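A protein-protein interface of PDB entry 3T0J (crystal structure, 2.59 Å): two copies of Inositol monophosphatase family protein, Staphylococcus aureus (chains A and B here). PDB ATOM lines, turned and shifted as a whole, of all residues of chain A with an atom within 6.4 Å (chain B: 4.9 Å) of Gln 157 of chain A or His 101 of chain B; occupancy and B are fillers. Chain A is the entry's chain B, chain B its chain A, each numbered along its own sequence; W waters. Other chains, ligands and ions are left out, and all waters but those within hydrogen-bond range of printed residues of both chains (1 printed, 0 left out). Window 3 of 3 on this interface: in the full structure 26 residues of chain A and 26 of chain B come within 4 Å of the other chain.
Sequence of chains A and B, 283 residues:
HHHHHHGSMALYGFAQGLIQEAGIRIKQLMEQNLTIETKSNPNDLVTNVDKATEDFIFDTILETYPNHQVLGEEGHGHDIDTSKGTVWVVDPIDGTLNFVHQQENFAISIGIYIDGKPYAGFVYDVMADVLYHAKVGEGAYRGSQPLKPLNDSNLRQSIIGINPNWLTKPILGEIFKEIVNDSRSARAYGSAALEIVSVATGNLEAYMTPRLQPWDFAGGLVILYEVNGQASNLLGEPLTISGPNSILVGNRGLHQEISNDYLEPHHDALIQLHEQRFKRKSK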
ATOM      1  N   SER A 153      16.865  35.531 -34.670  1.00  0.00           N
ATOM      2  CA  SER A 153      17.438  34.224 -34.381  1.00  0.00           C
ATOM      3  C   SER A 153      17.473  33.426 -35.661  1.00  0.00           C
ATOM      4  O   SER A 153      16.590  33.590 -36.490  1.00  0.00           O
ATOM      5  CB  SER A 153      16.589  33.475 -33.361  1.00  0.00           C
ATOM      6  OG  SER A 153      15.288  33.245 -33.873  1.00  0.00           O
ATOM      7  N   ASN A 154      18.487  32.576 -35.827  1.00  0.00           N
ATOM      8  CA  ASN A 154      18.530  31.583 -36.886  1.00  0.00           C
ATOM      9  C   ASN A 154      17.591  30.415 -36.541  1.00  0.00           C
ATOM     10  O   ASN A 154      17.516  30.008 -35.381  1.00  0.00           O
ATOM     11  CB  ASN A 154      19.970  31.067 -37.038  1.00  0.00           C
ATOM     12  CG  ASN A 154      20.965  32.185 -37.325  1.00  0.00           C
ATOM     13  OD1 ASN A 154      20.789  32.949 -38.275  1.00  0.00           O
ATOM     14  ND2 ASN A 154      22.026  32.271 -36.523  1.00  0.00           N
ATOM     15  N   LEU A 155      16.929  29.843 -37.546  1.00  0.00           N
ATOM     16  CA  LEU A 155      15.951  28.751 -37.324  1.00  0.00           C
ATOM     17  C   LEU A 155      16.556  27.570 -36.617  1.00  0.00           C
ATOM     18  O   LEU A 155      15.880  26.949 -35.797  1.00  0.00           O
ATOM     19  CB  LEU A 155      15.319  28.268 -38.643  1.00  0.00           C
ATOM     20  CG  LEU A 155      14.272  27.147 -38.526  1.00  0.00           C
ATOM     21  CD1 LEU A 155      12.989  27.560 -37.820  1.00  0.00           C
ATOM     22  CD2 LEU A 155      13.947  26.563 -39.885  1.00  0.00           C
ATOM     23  N   ARG A 156      17.806  27.246 -36.945  1.00  0.00           N
ATOM     24  CA  ARG A 156      18.514  26.109 -36.364  1.00  0.00           C
ATOM     25  C   ARG A 156      18.671  26.280 -34.856  1.00  0.00           C
ATOM     26  O   ARG A 156      18.889  25.309 -34.121  1.00  0.00           O
ATOM     27  CB  ARG A 156      19.901  25.932 -36.993  1.00  0.00           C
ATOM     28  CG  ARG A 156      19.883  25.090 -38.239  1.00  0.00           C
ATOM     29  CD  ARG A 156      21.274  24.729 -38.721  1.00  0.00           C
ATOM     30  NE  ARG A 156      21.258  23.965 -39.970  1.00  0.00           N
ATOM     31  CZ  ARG A 156      20.844  24.417 -41.171  1.00  0.00           C
ATOM     32  NH1 ARG A 156      20.375  25.642 -41.337  1.00  0.00           N
ATOM     33  NH2 ARG A 156      20.875  23.619 -42.214  1.00  0.00           N
ATOM     34  N   GLN A 157      18.544  27.524 -34.405  1.00  0.00           N
ATOM     35  CA  GLN A 157      18.762  27.840 -33.015  1.00  0.00           C
ATOM     36  C   GLN A 157      17.505  28.293 -32.332  1.00  0.00           C
ATOM     37  O   GLN A 157      17.572  28.832 -31.197  1.00  0.00           O
ATOM     38  CB  GLN A 157      19.817  28.919 -32.911  1.00  0.00           C
ATOM     39  CG  GLN A 157      21.134  28.357 -33.355  1.00  0.00           C
ATOM     40  CD  GLN A 157      22.224  29.390 -33.503  1.00  0.00           C
ATOM     41  OE1 GLN A 157      22.024  30.450 -34.108  1.00  0.00           O
ATOM     42  NE2 GLN A 157      23.408  29.065 -32.982  1.00  0.00           N
ATOM     43  N   SER A 158      16.373  28.063 -33.008  1.00  0.00           N
ATOM     44  CA  SER A 158      15.110  28.633 -32.597  1.00  0.00           C
ATOM     45  C   SER A 158      14.201  27.526 -32.104  1.00  0.00           C
ATOM     46  O   SER A 158      14.196  26.394 -32.647  1.00  0.00           O
ATOM     47  CB  SER A 158      14.457  29.361 -33.756  1.00  0.00           C
ATOM     48  OG  SER A 158      15.179  30.523 -34.133  1.00  0.00           O
ATOM     49  N   ILE A 159      13.428  27.816 -31.064  1.00  0.00           N
ATOM     50  CA  ILE A 159      12.372  26.875 -30.684  1.00  0.00           C
ATOM     51  C   ILE A 159      11.092  27.387 -31.263  1.00  0.00           C
ATOM     52  O   ILE A 159      10.834  28.601 -31.251  1.00  0.00           O
ATOM     53  CB  ILE A 159      12.200  26.719 -29.196  1.00  0.00           C
ATOM     54  CG1 ILE A 159      13.510  26.305 -28.558  1.00  0.00           C
ATOM     55  CG2 ILE A 159      11.178  25.647 -28.945  1.00  0.00           C
ATOM     56  CD1 ILE A 159      13.333  25.728 -27.183  1.00  0.00           C
ATOM     57  N   ASP A 182      14.569  21.120 -38.916  1.00  0.00           N
ATOM     58  CA  ASP A 182      15.620  22.074 -38.934  1.00  0.00           C
ATOM     59  C   ASP A 182      15.805  22.933 -37.682  1.00  0.00           C
ATOM     60  O   ASP A 182      16.946  23.280 -37.331  1.00  0.00           O
ATOM     61  CB  ASP A 182      15.273  22.996 -40.041  1.00  0.00           C
ATOM     62  CG  ASP A 182      16.412  23.358 -40.772  1.00  0.00           C
ATOM     63  OD1 ASP A 182      16.952  22.430 -41.450  1.00  0.00           O
ATOM     64  OD2 ASP A 182      16.775  24.548 -40.610  1.00  0.00           O
ATOM     65  N   SER A 183      14.679  23.307 -37.054  1.00  0.00           N
ATOM     66  CA  SER A 183      14.672  24.187 -35.899  1.00  0.00           C
ATOM     67  C   SER A 183      15.267  23.453 -34.682  1.00  0.00           C
ATOM     68  O   SER A 183      15.517  22.277 -34.748  1.00  0.00           O
ATOM     69  CB  SER A 183      13.252  24.664 -35.654  1.00  0.00           C
ATOM     70  OG  SER A 183      12.394  23.551 -35.543  1.00  0.00           O
ATOM     71  N   ARG A 184      15.546  24.117 -33.582  1.00  0.00           N
ATOM     72  CA  ARG A 184      16.315  23.429 -32.540  1.00  0.00           C
ATOM     73  C   ARG A 184      15.416  22.374 -31.899  1.00  0.00           C
ATOM     74  O   ARG A 184      15.835  21.220 -31.720  1.00  0.00           O
ATOM     75  CB  ARG A 184      16.890  24.451 -31.558  1.00  0.00           C
ATOM     76  CG  ARG A 184      17.753  23.996 -30.426  1.00  0.00           C
ATOM     77  CD  ARG A 184      19.006  23.238 -30.787  1.00  0.00           C
ATOM     78  NE  ARG A 184      18.699  21.862 -30.468  1.00  0.00           N
ATOM     79  CZ  ARG A 184      19.248  21.130 -29.509  1.00  0.00           C
ATOM     80  NH1 ARG A 184      20.263  21.578 -28.779  1.00  0.00           N
ATOM     81  NH2 ARG A 184      18.779  19.904 -29.312  1.00  0.00           N
ATOM     82  N   THR A 201       7.163  37.284 -25.512  1.00  0.00           N
ATOM     83  CA  THR A 201       8.045  37.222 -24.323  1.00  0.00           C
ATOM     84  C   THR A 201       9.463  36.625 -24.531  1.00  0.00           C
ATOM     85  O   THR A 201      10.308  36.690 -23.628  1.00  0.00           O
ATOM     86  CB  THR A 201       7.390  36.504 -23.117  1.00  0.00           C
ATOM     87  OG1 THR A 201       7.294  35.093 -23.364  1.00  0.00           O
ATOM     88  CG2 THR A 201       6.036  37.085 -22.847  1.00  0.00           C
ATOM     89  N   GLY A 202       9.712  36.072 -25.719  1.00  0.00           N
ATOM     90  CA  GLY A 202      10.901  35.269 -25.982  1.00  0.00           C
ATOM     91  C   GLY A 202      10.856  33.812 -25.516  1.00  0.00           C
ATOM     92  O   GLY A 202      11.868  33.154 -25.551  1.00  0.00           O
ATOM     93  N   ASN A 203       9.714  33.289 -25.068  1.00  0.00           N
ATOM     94  CA  ASN A 203       9.640  31.859 -24.730  1.00  0.00           C
ATOM     95  C   ASN A 203       9.643  30.908 -25.925  1.00  0.00           C
ATOM     96  O   ASN A 203      10.108  29.774 -25.814  1.00  0.00           O
ATOM     97  CB  ASN A 203       8.456  31.549 -23.820  1.00  0.00           C
ATOM     98  CG  ASN A 203       8.843  31.582 -22.337  1.00  0.00           C
ATOM     99  OD1 ASN A 203       9.827  32.245 -21.948  1.00  0.00           O
ATOM    100  ND2 ASN A 203       8.090  30.842 -21.501  1.00  0.00           N
ATOM    101  N   LEU A 204       9.081  31.374 -27.039  1.00  0.00           N
ATOM    102  CA  LEU A 204       9.233  30.743 -28.342  1.00  0.00           C
ATOM    103  C   LEU A 204       9.883  31.776 -29.283  1.00  0.00           C
ATOM    104  O   LEU A 204       9.654  32.980 -29.111  1.00  0.00           O
ATOM    105  CB  LEU A 204       7.871  30.292 -28.898  1.00  0.00           C
ATOM    106  CG  LEU A 204       7.192  29.284 -27.991  1.00  0.00           C
ATOM    107  CD1 LEU A 204       5.836  28.887 -28.488  1.00  0.00           C
ATOM    108  CD2 LEU A 204       8.108  28.089 -27.892  1.00  0.00           C
ATOM    109  N   GLU A 205      10.680  31.313 -30.250  1.00  0.00           N
ATOM    110  CA  GLU A 205      11.189  32.187 -31.303  1.00  0.00           C
ATOM    111  C   GLU A 205      10.169  32.342 -32.422  1.00  0.00           C
ATOM    112  O   GLU A 205      10.083  33.389 -33.052  1.00  0.00           O
ATOM    113  CB  GLU A 205      12.521  31.685 -31.867  1.00  0.00           C
ATOM    114  CG  GLU A 205      13.696  32.114 -31.065  1.00  0.00           C
ATOM    115  CD  GLU A 205      13.914  31.313 -29.766  1.00  0.00           C
ATOM    116  OE1 GLU A 205      13.554  30.115 -29.645  1.00  0.00           O
ATOM    117  OE2 GLU A 205      14.504  31.897 -28.846  1.00  0.00           O
ATOM    118  N   LEU B  97      17.087  22.976 -22.855  1.00  0.00           N
ATOM    119  CA  LEU B  97      16.634  23.930 -23.862  1.00  0.00           C
ATOM    120  C   LEU B  97      15.668  24.988 -23.284  1.00  0.00           C
ATOM    121  O   LEU B  97      15.828  26.203 -23.516  1.00  0.00           O
ATOM    122  CB  LEU B  97      16.046  23.222 -25.059  1.00  0.00           C
ATOM    123  CG  LEU B  97      17.070  22.827 -26.124  1.00  0.00           C
ATOM    124  CD1 LEU B  97      16.379  22.258 -27.369  1.00  0.00           C
ATOM    125  CD2 LEU B  97      18.037  24.034 -26.530  1.00  0.00           C
ATOM    126  N   ASN B  98      14.706  24.531 -22.494  1.00  0.00           N
ATOM    127  CA  ASN B  98      13.781  25.428 -21.821  1.00  0.00           C
ATOM    128  C   ASN B  98      14.508  26.377 -20.864  1.00  0.00           C
ATOM    129  O   ASN B  98      14.161  27.565 -20.789  1.00  0.00           O
ATOM    130  CB  ASN B  98      12.712  24.635 -21.065  1.00  0.00           C
ATOM    131  CG  ASN B  98      11.677  24.018 -21.984  1.00  0.00           C
ATOM    132  OD1 ASN B  98      11.496  24.426 -23.146  1.00  0.00           O
ATOM    133  ND2 ASN B  98      10.969  23.027 -21.459  1.00  0.00           N
ATOM    134  N   PHE B  99      15.514  25.854 -20.155  1.00  0.00           N
ATOM    135  CA  PHE B  99      16.349  26.683 -19.305  1.00  0.00           C
ATOM    136  C   PHE B  99      17.036  27.733 -20.161  1.00  0.00           C
ATOM    137  O   PHE B  99      17.089  28.907 -19.785  1.00  0.00           O
ATOM    138  CB  PHE B  99      17.376  25.844 -18.556  1.00  0.00           C
ATOM    139  CG  PHE B  99      18.313  26.639 -17.697  1.00  0.00           C
ATOM    140  CD1 PHE B  99      18.176  26.626 -16.311  1.00  0.00           C
ATOM    141  CD2 PHE B  99      19.381  27.396 -18.279  1.00  0.00           C
ATOM    142  CE1 PHE B  99      19.050  27.356 -15.488  1.00  0.00           C
ATOM    143  CE2 PHE B  99      20.277  28.132 -17.477  1.00  0.00           C
ATOM    144  CZ  PHE B  99      20.108  28.110 -16.065  1.00  0.00           C
ATOM    145  N   VAL B 100      17.540  27.345 -21.323  1.00  0.00           N
ATOM    146  CA  VAL B 100      18.367  28.312 -22.052  1.00  0.00           C
ATOM    147  C   VAL B 100      17.477  29.372 -22.654  1.00  0.00           C
ATOM    148  O   VAL B 100      17.808  30.547 -22.601  1.00  0.00           O
ATOM    149  CB  VAL B 100      19.320  27.649 -23.106  1.00  0.00           C
ATOM    150  CG1 VAL B 100      20.007  28.700 -23.999  1.00  0.00           C
ATOM    151  CG2 VAL B 100      20.367  26.833 -22.394  1.00  0.00           C
ATOM    152  N   HIS B 101      16.334  28.949 -23.178  1.00  0.00           N
ATOM    153  CA  HIS B 101      15.453  29.821 -23.975  1.00  0.00           C
ATOM    154  C   HIS B 101      14.312  30.495 -23.245  1.00  0.00           C
ATOM    155  O   HIS B 101      13.902  31.604 -23.617  1.00  0.00           O
ATOM    156  CB  HIS B 101      14.850  29.031 -25.122  1.00  0.00           C
ATOM    157  CG  HIS B 101      15.840  28.693 -26.174  1.00  0.00           C
ATOM    158  ND1 HIS B 101      16.185  29.579 -27.170  1.00  0.00           N
ATOM    159  CD2 HIS B 101      16.601  27.591 -26.361  1.00  0.00           C
ATOM    160  CE1 HIS B 101      17.105  29.027 -27.940  1.00  0.00           C
ATOM    161  NE2 HIS B 101      17.386  27.827 -27.462  1.00  0.00           N
ATOM    162  N   GLN B 102      13.775  29.806 -22.242  1.00  0.00           N
ATOM    163  CA  GLN B 102      12.580  30.261 -21.540  1.00  0.00           C
ATOM    164  C   GLN B 102      12.873  30.754 -20.116  1.00  0.00           C
ATOM    165  O   GLN B 102      12.014  31.390 -19.502  1.00  0.00           O
ATOM    166  CB  GLN B 102      11.515  29.148 -21.540  1.00  0.00           C
ATOM    167  CG  GLN B 102      11.286  28.539 -22.895  1.00  0.00           C
ATOM    168  CD  GLN B 102      10.085  27.575 -22.967  1.00  0.00           C
ATOM    169  OE1 GLN B 102       9.893  26.728 -22.093  1.00  0.00           O
ATOM    170  NE2 GLN B 102       9.309  27.670 -24.052  1.00  0.00           N
ATOM    171  N   GLN B 103      14.087  30.462 -19.625  1.00  0.00           N
ATOM    172  CA  GLN B 103      14.512  30.653 -18.216  1.00  0.00           C
ATOM    173  C   GLN B 103      13.531  30.085 -17.226  1.00  0.00           C
ATOM    174  O   GLN B 103      13.318  30.679 -16.154  1.00  0.00           O
ATOM    175  CB  GLN B 103      14.732  32.123 -17.844  1.00  0.00           C
ATOM    176  CG  GLN B 103      16.004  32.711 -18.388  1.00  0.00           C
ATOM    177  CD  GLN B 103      15.999  32.661 -19.894  1.00  0.00           C
ATOM    178  OE1 GLN B 103      15.182  33.338 -20.558  1.00  0.00           O
ATOM    179  NE2 GLN B 103      16.874  31.817 -20.455  1.00  0.00           N
HETATM  180  O   HOH W   1      17.075  32.446 -28.790  1.00  0.00           O
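ND1 of His 101 of chain B sits at hydrogen-bond distance from OE2 of Glu 205 of chain A, 3.3 Å away. NE2 of Gln 102 of chain B is in hydrogen-bond range of O of Asn 203 of chain A (2.9 Å). The backbone carbonyl oxygen (O) of Gly 202 of chain A lies close to the backbone carbonyl oxygen (O) of His 101 of chain B.
The side-chain amide oxygen (OD1) of Asn 98 of chain B sits close to the side-chain amide oxygen (OE1) of Gln 102 of chain B (3.0 Å). The side-chain amide nitrogen of Asn 154 of chain A lies within hydrogen-bond range of the side-chain amide oxygen of Gln 157 of chain A (3.0 Å). The backbone NH (N) of Arg 184 of chain A is in hydrogen-bond range of the backbone carbonyl oxygen (O) of Ser 158 of chain A, 2.8 Å away. The backbone NH (N) of Ile 159 of chain A lies within hydrogen-bond range of the side-chain carboxylate (OE1) of Glu 205 of chain A (2.7 Å). OG1 of Thr 201 of chain A sits close to N of Asn 203 of chain A (3.5 Å).
Gln 157 of chain A touches His 101 of chain B. Ile 159 of chain A touches His 101 of chain B. Leu 97 of chain B touches Arg 184 of chain A (CD1 to CZ, 3.8 Å).
Of chain B, only His 101 comes within 4 Å of Gln 157 of chain A. Of the printed residues of chain B, Ile 159 of chain A touches His 101. His 101 of chain B touches four residues of chain A. Of the printed residues of chain A, Gln 102 of chain B touches Asn 203 (2.9 Å).
Printed residues of chain A that touch a printed residue of chain B: Gln 157, Ile 159, Arg 184, Gly 202, Asn 203 and Glu 205. Hydrophobic or aromatic side chains of chain A within 4 Å of the printed part of chain B: Ile 159. Of the 7 printed residues of chain B, 3 touch a printed residue of chain A. Hydrophobic or aromatic side chains of chain B within 4 Å of the printed part of chain A: Leu 97 and His 101. Among the printed residues, 6 pairs touch across the chains. Among the printed residues, no Asp or Glu carboxylate lies within 4 Å of a Lys or Arg side-chain nitrogen of the other chain.
No position is printed for both chains. Of the 6 pairs that touch across the chains among the printed residues, none has its exchanged pair printed and touching as well.
Water W1 bridges the side-chain carboxylate (OE2) of Glu 205 of chain A and a ring nitrogen (ND1) of His 101 of chain B.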
